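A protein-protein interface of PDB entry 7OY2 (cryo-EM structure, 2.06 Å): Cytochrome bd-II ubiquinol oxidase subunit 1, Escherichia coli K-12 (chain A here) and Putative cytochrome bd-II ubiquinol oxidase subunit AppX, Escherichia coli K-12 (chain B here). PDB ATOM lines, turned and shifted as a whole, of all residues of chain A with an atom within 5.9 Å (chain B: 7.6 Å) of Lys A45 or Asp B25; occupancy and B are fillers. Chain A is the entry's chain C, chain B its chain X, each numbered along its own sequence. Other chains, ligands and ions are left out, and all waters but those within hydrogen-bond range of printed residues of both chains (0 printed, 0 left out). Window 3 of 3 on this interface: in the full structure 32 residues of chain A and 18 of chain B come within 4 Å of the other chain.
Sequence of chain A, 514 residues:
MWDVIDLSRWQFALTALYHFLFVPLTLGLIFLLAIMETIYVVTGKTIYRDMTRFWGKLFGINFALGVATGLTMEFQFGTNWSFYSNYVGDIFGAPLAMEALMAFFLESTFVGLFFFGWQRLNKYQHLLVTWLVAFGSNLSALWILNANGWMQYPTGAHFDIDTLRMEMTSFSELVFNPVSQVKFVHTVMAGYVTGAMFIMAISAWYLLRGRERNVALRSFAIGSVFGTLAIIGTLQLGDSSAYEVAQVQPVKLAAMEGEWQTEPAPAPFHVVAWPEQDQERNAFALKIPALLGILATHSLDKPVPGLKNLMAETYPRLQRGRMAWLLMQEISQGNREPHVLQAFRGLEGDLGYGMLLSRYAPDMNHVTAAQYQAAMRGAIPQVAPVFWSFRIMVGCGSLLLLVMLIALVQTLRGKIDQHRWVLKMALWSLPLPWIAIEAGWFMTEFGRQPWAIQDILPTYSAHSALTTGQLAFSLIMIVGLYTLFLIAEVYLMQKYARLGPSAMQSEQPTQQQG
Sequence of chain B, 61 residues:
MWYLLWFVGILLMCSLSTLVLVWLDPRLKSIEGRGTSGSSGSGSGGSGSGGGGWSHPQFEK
Of the 10 printed residues of chain B, 4 touch a printed residue of chain A.
Hydrophobic or aromatic side chains of chain B within 4 Å of the printed part of chain A: Leu B21, Val B22 and Leu B28.
Among the printed residues, 7 pairs touch across the chains.
CB of Leu B21 touches CD1 of Ile A39 (3.5 Å).
Val B22 touches Thr A43.
Leu B21 touches Tyr A48.
CD1 of Leu B28 touches CG of Arg A218 (3.8 Å).
Of chain B, only Asp B25 (3.3 Å) comes within 4 Å of Lys A45.
Of chain A, only Lys A45 (3.3 Å), Tyr A48 (2.4 Å) and Arg A218 (3.1 Å) come within 4 Å of Asp B25.
No residue of chain B comes within 4 Å of Gly A44.
Of the printed residues of chain B, Thr A43 touches Val B22 (3.7 Å).
Of the printed residues of chain A, Leu B21 touches Ile A39 (3.5 Å) and Tyr A48 (3.6 Å).
Of the printed residues of chain B, Arg A218 touches Asp B25 (3.1 Å) and Leu B28 (3.8 Å).
Of the printed residues of chain A, Val B22 touches Thr A43 (3.7 Å).
Of the printed residues of chain B, Ile A39 touches Leu B21.
Trp B23 touches none of the printed residues of chain A.
Arg A49 touches none of the printed residues of chain B.
The side-chain carboxylate of Asp B25 is in salt-bridge range of the side-chain amino group of Lys A45 (3.4 Å).
NE of Arg A218 is in salt-bridge range of OD2 of Asp B25 (3.1 Å).
The side-chain hydroxyl (OH) of Tyr A48 lies close to the side-chain carboxylate (OD2) of Asp B25.
The side-chain hydroxyl (OG1) of Thr A43 is in hydrogen-bond range of the backbone carbonyl oxygen (O) of Ile A39, at 2.8 Å.
The side-chain hydroxyl (OG1) of Thr A43 sits close to the backbone NH (N) of Lys A45 (3.1 Å).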
ATOM      1  N   ILE A  39      14.234  10.044  23.235  1.00  0.00           N
ATOM      2  CA  ILE A  39      15.038  10.996  23.996  1.00  0.00           C
ATOM      3  C   ILE A  39      15.758  10.277  25.127  1.00  0.00           C
ATOM      4  O   ILE A  39      16.937  10.536  25.398  1.00  0.00           O
ATOM      5  CB  ILE A  39      14.171  12.154  24.525  1.00  0.00           C
ATOM      6  CG1 ILE A  39      13.589  12.974  23.380  1.00  0.00           C
ATOM      7  CG2 ILE A  39      14.997  13.073  25.425  1.00  0.00           C
ATOM      8  CD1 ILE A  39      12.393  13.782  23.786  1.00  0.00           C
ATOM      9  N   TYR A  40      15.063   9.346  25.785  1.00  0.00           N
ATOM     10  CA  TYR A  40      15.688   8.563  26.843  1.00  0.00           C
ATOM     11  C   TYR A  40      16.866   7.756  26.309  1.00  0.00           C
ATOM     12  O   TYR A  40      17.904   7.643  26.972  1.00  0.00           O
ATOM     13  CB  TYR A  40      14.658   7.635  27.489  1.00  0.00           C
ATOM     14  CG  TYR A  40      15.273   6.525  28.309  1.00  0.00           C
ATOM     15  CD1 TYR A  40      16.091   6.807  29.395  1.00  0.00           C
ATOM     16  CD2 TYR A  40      15.046   5.193  27.989  1.00  0.00           C
ATOM     17  CE1 TYR A  40      16.656   5.798  30.141  1.00  0.00           C
ATOM     18  CE2 TYR A  40      15.610   4.176  28.731  1.00  0.00           C
ATOM     19  CZ  TYR A  40      16.415   4.484  29.810  1.00  0.00           C
ATOM     20  OH  TYR A  40      16.982   3.477  30.556  1.00  0.00           O
ATOM     21  N   THR A  43      19.834  10.328  25.276  1.00  0.00           N
ATOM     22  CA  THR A  43      20.462  11.065  26.362  1.00  0.00           C
ATOM     23  C   THR A  43      20.800  10.225  27.582  1.00  0.00           C
ATOM     24  O   THR A  43      21.642  10.645  28.381  1.00  0.00           O
ATOM     25  CB  THR A  43      19.558  12.224  26.813  1.00  0.00           C
ATOM     26  OG1 THR A  43      18.388  11.701  27.453  1.00  0.00           O
ATOM     27  CG2 THR A  43      19.136  13.057  25.627  1.00  0.00           C
ATOM     28  N   GLY A  44      20.172   9.067  27.754  1.00  0.00           N
ATOM     29  CA  GLY A  44      20.340   8.313  28.975  1.00  0.00           C
ATOM     30  C   GLY A  44      19.662   8.909  30.186  1.00  0.00           C
ATOM     31  O   GLY A  44      19.849   8.394  31.295  1.00  0.00           O
ATOM     32  N   LYS A  45      18.879   9.972  30.012  1.00  0.00           N
ATOM     33  CA  LYS A  45      18.222  10.654  31.121  1.00  0.00           C
ATOM     34  C   LYS A  45      16.975   9.872  31.518  1.00  0.00           C
ATOM     35  O   LYS A  45      16.054   9.705  30.714  1.00  0.00           O
ATOM     36  CB  LYS A  45      17.885  12.088  30.724  1.00  0.00           C
ATOM     37  CG  LYS A  45      18.847  13.118  31.289  1.00  0.00           C
ATOM     38  CD  LYS A  45      18.872  14.381  30.456  1.00  0.00           C
ATOM     39  CE  LYS A  45      20.213  14.557  29.759  1.00  0.00           C
ATOM     40  NZ  LYS A  45      20.390  15.936  29.231  1.00  0.00           N
ATOM     41  N   THR A  46      16.950   9.395  32.763  1.00  0.00           N
ATOM     42  CA  THR A  46      15.909   8.469  33.201  1.00  0.00           C
ATOM     43  C   THR A  46      14.541   9.132  33.274  1.00  0.00           C
ATOM     44  O   THR A  46      13.515   8.438  33.227  1.00  0.00           O
ATOM     45  CB  THR A  46      16.268   7.893  34.566  1.00  0.00           C
ATOM     46  OG1 THR A  46      16.423   8.963  35.508  1.00  0.00           O
ATOM     47  CG2 THR A  46      17.562   7.107  34.488  1.00  0.00           C
ATOM     48  N   ILE A  47      14.503  10.458  33.408  1.00  0.00           N
ATOM     49  CA  ILE A  47      13.225  11.145  33.557  1.00  0.00           C
ATOM     50  C   ILE A  47      12.345  10.887  32.342  1.00  0.00           C
ATOM     51  O   ILE A  47      11.122  10.783  32.457  1.00  0.00           O
ATOM     52  CB  ILE A  47      13.445  12.650  33.806  1.00  0.00           C
ATOM     53  CG1 ILE A  47      12.099  13.368  33.965  1.00  0.00           C
ATOM     54  CG2 ILE A  47      14.271  13.277  32.697  1.00  0.00           C
ATOM     55  CD1 ILE A  47      12.154  14.555  34.887  1.00  0.00           C
ATOM     56  N   TYR A  48      12.954  10.731  31.165  1.00  0.00           N
ATOM     57  CA  TYR A  48      12.169  10.446  29.970  1.00  0.00           C
ATOM     58  C   TYR A  48      11.651   9.012  29.957  1.00  0.00           C
ATOM     59  O   TYR A  48      10.575   8.756  29.414  1.00  0.00           O
ATOM     60  CB  TYR A  48      12.991  10.752  28.721  1.00  0.00           C
ATOM     61  CG  TYR A  48      13.240  12.229  28.566  1.00  0.00           C
ATOM     62  CD1 TYR A  48      12.297  13.050  27.968  1.00  0.00           C
ATOM     63  CD2 TYR A  48      14.397  12.810  29.054  1.00  0.00           C
ATOM     64  CE1 TYR A  48      12.513  14.401  27.839  1.00  0.00           C
ATOM     65  CE2 TYR A  48      14.620  14.160  28.934  1.00  0.00           C
ATOM     66  CZ  TYR A  48      13.676  14.950  28.321  1.00  0.00           C
ATOM     67  OH  TYR A  48      13.892  16.300  28.194  1.00  0.00           O
ATOM     68  N   ARG A  49      12.385   8.070  30.558  1.00  0.00           N
ATOM     69  CA  ARG A  49      11.851   6.723  30.749  1.00  0.00           C
ATOM     70  C   ARG A  49      10.650   6.738  31.688  1.00  0.00           C
ATOM     71  O   ARG A  49       9.616   6.116  31.404  1.00  0.00           O
ATOM     72  CB  ARG A  49      12.942   5.798  31.290  1.00  0.00           C
ATOM     73  CG  ARG A  49      12.485   4.368  31.530  1.00  0.00           C
ATOM     74  CD  ARG A  49      13.580   3.535  32.177  1.00  0.00           C
ATOM     75  NE  ARG A  49      13.831   3.926  33.560  1.00  0.00           N
ATOM     76  CZ  ARG A  49      14.943   3.632  34.230  1.00  0.00           C
ATOM     77  NH1 ARG A  49      15.092   4.024  35.487  1.00  0.00           N
ATOM     78  NH2 ARG A  49      15.914   2.954  33.635  1.00  0.00           N
ATOM     79  N   ARG A 218       9.102  18.939  30.950  1.00  0.00           N
ATOM     80  CA  ARG A 218       9.566  18.221  29.769  1.00  0.00           C
ATOM     81  C   ARG A 218       8.394  17.736  28.918  1.00  0.00           C
ATOM     82  O   ARG A 218       8.451  17.798  27.684  1.00  0.00           O
ATOM     83  CB  ARG A 218      10.459  17.055  30.180  1.00  0.00           C
ATOM     84  CG  ARG A 218      11.841  17.456  30.647  1.00  0.00           C
ATOM     85  CD  ARG A 218      12.351  16.485  31.689  1.00  0.00           C
ATOM     86  NE  ARG A 218      13.734  16.754  32.065  1.00  0.00           N
ATOM     87  CZ  ARG A 218      14.119  17.750  32.855  1.00  0.00           C
ATOM     88  NH1 ARG A 218      13.230  18.590  33.361  1.00  0.00           N
ATOM     89  NH2 ARG A 218      15.403  17.906  33.134  1.00  0.00           N
ATOM     90  N   LEU B  19      15.401  16.288  19.029  1.00  0.00           N
ATOM     91  CA  LEU B  19      16.533  17.207  18.990  1.00  0.00           C
ATOM     92  C   LEU B  19      16.268  18.456  19.821  1.00  0.00           C
ATOM     93  O   LEU B  19      17.152  18.924  20.549  1.00  0.00           O
ATOM     94  CB  LEU B  19      16.848  17.586  17.542  1.00  0.00           C
ATOM     95  CG  LEU B  19      17.609  16.553  16.708  1.00  0.00           C
ATOM     96  CD1 LEU B  19      17.668  16.986  15.252  1.00  0.00           C
ATOM     97  CD2 LEU B  19      19.009  16.316  17.259  1.00  0.00           C
ATOM     98  N   VAL B  20      15.060  19.015  19.724  1.00  0.00           N
ATOM     99  CA  VAL B  20      14.722  20.197  20.504  1.00  0.00           C
ATOM    100  C   VAL B  20      14.755  19.880  21.992  1.00  0.00           C
ATOM    101  O   VAL B  20      15.200  20.700  22.800  1.00  0.00           O
ATOM    102  CB  VAL B  20      13.356  20.755  20.069  1.00  0.00           C
ATOM    103  CG1 VAL B  20      12.794  21.674  21.135  1.00  0.00           C
ATOM    104  CG2 VAL B  20      13.480  21.492  18.753  1.00  0.00           C
ATOM    105  N   LEU B  21      14.306  18.686  22.382  1.00  0.00           N
ATOM    106  CA  LEU B  21      14.337  18.344  23.799  1.00  0.00           C
ATOM    107  C   LEU B  21      15.756  18.071  24.276  1.00  0.00           C
ATOM    108  O   LEU B  21      16.096  18.373  25.425  1.00  0.00           O
ATOM    109  CB  LEU B  21      13.428  17.152  24.077  1.00  0.00           C
ATOM    110  CG  LEU B  21      12.027  17.543  24.554  1.00  0.00           C
ATOM    111  CD1 LEU B  21      12.080  18.347  25.851  1.00  0.00           C
ATOM    112  CD2 LEU B  21      11.271  18.304  23.484  1.00  0.00           C
ATOM    113  N   VAL B  22      16.598  17.495  23.416  1.00  0.00           N
ATOM    114  CA  VAL B  22      18.001  17.306  23.769  1.00  0.00           C
ATOM    115  C   VAL B  22      18.672  18.655  23.985  1.00  0.00           C
ATOM    116  O   VAL B  22      19.422  18.849  24.948  1.00  0.00           O
ATOM    117  CB  VAL B  22      18.717  16.475  22.686  1.00  0.00           C
ATOM    118  CG1 VAL B  22      20.208  16.444  22.936  1.00  0.00           C
ATOM    119  CG2 VAL B  22      18.159  15.060  22.651  1.00  0.00           C
ATOM    120  N   TRP B  23      18.399  19.610  23.098  1.00  0.00           N
ATOM    121  CA  TRP B  23      18.965  20.947  23.234  1.00  0.00           C
ATOM    122  C   TRP B  23      18.437  21.654  24.475  1.00  0.00           C
ATOM    123  O   TRP B  23      19.198  22.282  25.218  1.00  0.00           O
ATOM    124  CB  TRP B  23      18.652  21.763  21.981  1.00  0.00           C
ATOM    125  CG  TRP B  23      18.819  23.234  22.159  1.00  0.00           C
ATOM    126  CD1 TRP B  23      19.991  23.912  22.318  1.00  0.00           C
ATOM    127  CD2 TRP B  23      17.777  24.217  22.197  1.00  0.00           C
ATOM    128  NE1 TRP B  23      19.744  25.255  22.452  1.00  0.00           N
ATOM    129  CE2 TRP B  23      18.393  25.469  22.384  1.00  0.00           C
ATOM    130  CE3 TRP B  23      16.383  24.160  22.093  1.00  0.00           C
ATOM    131  CZ2 TRP B  23      17.665  26.654  22.465  1.00  0.00           C
ATOM    132  CZ3 TRP B  23      15.661  25.338  22.175  1.00  0.00           C
ATOM    133  CH2 TRP B  23      16.303  26.567  22.360  1.00  0.00           C
ATOM    134  N   LEU B  24      17.132  21.558  24.717  1.00  0.00           N
ATOM    135  CA  LEU B  24      16.475  22.376  25.725  1.00  0.00           C
ATOM    136  C   LEU B  24      16.554  21.776  27.122  1.00  0.00           C
ATOM    137  O   LEU B  24      16.394  22.509  28.104  1.00  0.00           O
ATOM    138  CB  LEU B  24      15.018  22.592  25.313  1.00  0.00           C
ATOM    139  CG  LEU B  24      14.124  23.504  26.147  1.00  0.00           C
ATOM    140  CD1 LEU B  24      14.146  24.905  25.557  1.00  0.00           C
ATOM    141  CD2 LEU B  24      12.715  22.937  26.162  1.00  0.00           C
ATOM    142  N   ASP B  25      16.812  20.475  27.230  1.00  0.00           N
ATOM    143  CA  ASP B  25      16.800  19.818  28.534  1.00  0.00           C
ATOM    144  C   ASP B  25      17.733  20.460  29.558  1.00  0.00           C
ATOM    145  O   ASP B  25      17.319  20.591  30.723  1.00  0.00           O
ATOM    146  CB  ASP B  25      17.122  18.330  28.359  1.00  0.00           C
ATOM    147  CG  ASP B  25      16.775  17.516  29.580  1.00  0.00           C
ATOM    148  OD1 ASP B  25      17.629  17.399  30.478  1.00  0.00           O
ATOM    149  OD2 ASP B  25      15.644  16.996  29.640  1.00  0.00           O
ATOM    150  N   PRO B  26      18.975  20.842  29.230  1.00  0.00           N
ATOM    151  CA  PRO B  26      19.785  21.564  30.228  1.00  0.00           C
ATOM    152  C   PRO B  26      19.150  22.856  30.716  1.00  0.00           C
ATOM    153  O   PRO B  26      19.265  23.188  31.901  1.00  0.00           O
ATOM    154  CB  PRO B  26      21.096  21.824  29.474  1.00  0.00           C
ATOM    155  CG  PRO B  26      21.204  20.682  28.553  1.00  0.00           C
ATOM    156  CD  PRO B  26      19.797  20.428  28.078  1.00  0.00           C
ATOM    157  N   ARG B  27      18.481  23.598  29.833  1.00  0.00           N
ATOM    158  CA  ARG B  27      17.825  24.835  30.246  1.00  0.00           C
ATOM    159  C   ARG B  27      16.675  24.554  31.208  1.00  0.00           C
ATOM    160  O   ARG B  27      16.447  25.310  32.158  1.00  0.00           O
ATOM    161  CB  ARG B  27      17.351  25.599  29.009  1.00  0.00           C
ATOM    162  CG  ARG B  27      18.465  25.803  27.989  1.00  0.00           C
ATOM    163  CD  ARG B  27      17.980  26.415  26.691  1.00  0.00           C
ATOM    164  NE  ARG B  27      19.099  26.753  25.818  1.00  0.00           N
ATOM    165  CZ  ARG B  27      19.517  27.992  25.575  1.00  0.00           C
ATOM    166  NH1 ARG B  27      18.890  29.025  26.118  1.00  0.00           N
ATOM    167  NH2 ARG B  27      20.553  28.197  24.771  1.00  0.00           N
ATOM    168  N   LEU B  28      15.943  23.469  30.980  1.00  0.00           N
ATOM    169  CA  LEU B  28      14.880  23.059  31.893  1.00  0.00           C
ATOM    170  C   LEU B  28      15.466  22.623  33.232  1.00  0.00           C
ATOM    171  O   LEU B  28      15.157  23.120  34.316  1.00  0.00           O
ATOM    172  CB  LEU B  28      14.049  21.927  31.287  1.00  0.00           C
ATOM    173  CG  LEU B  28      13.400  22.210  29.931  1.00  0.00           C
ATOM    174  CD1 LEU B  28      12.693  20.971  29.393  1.00  0.00           C
ATOM    175  CD2 LEU B  28      12.436  23.372  30.036  1.00  0.00           C
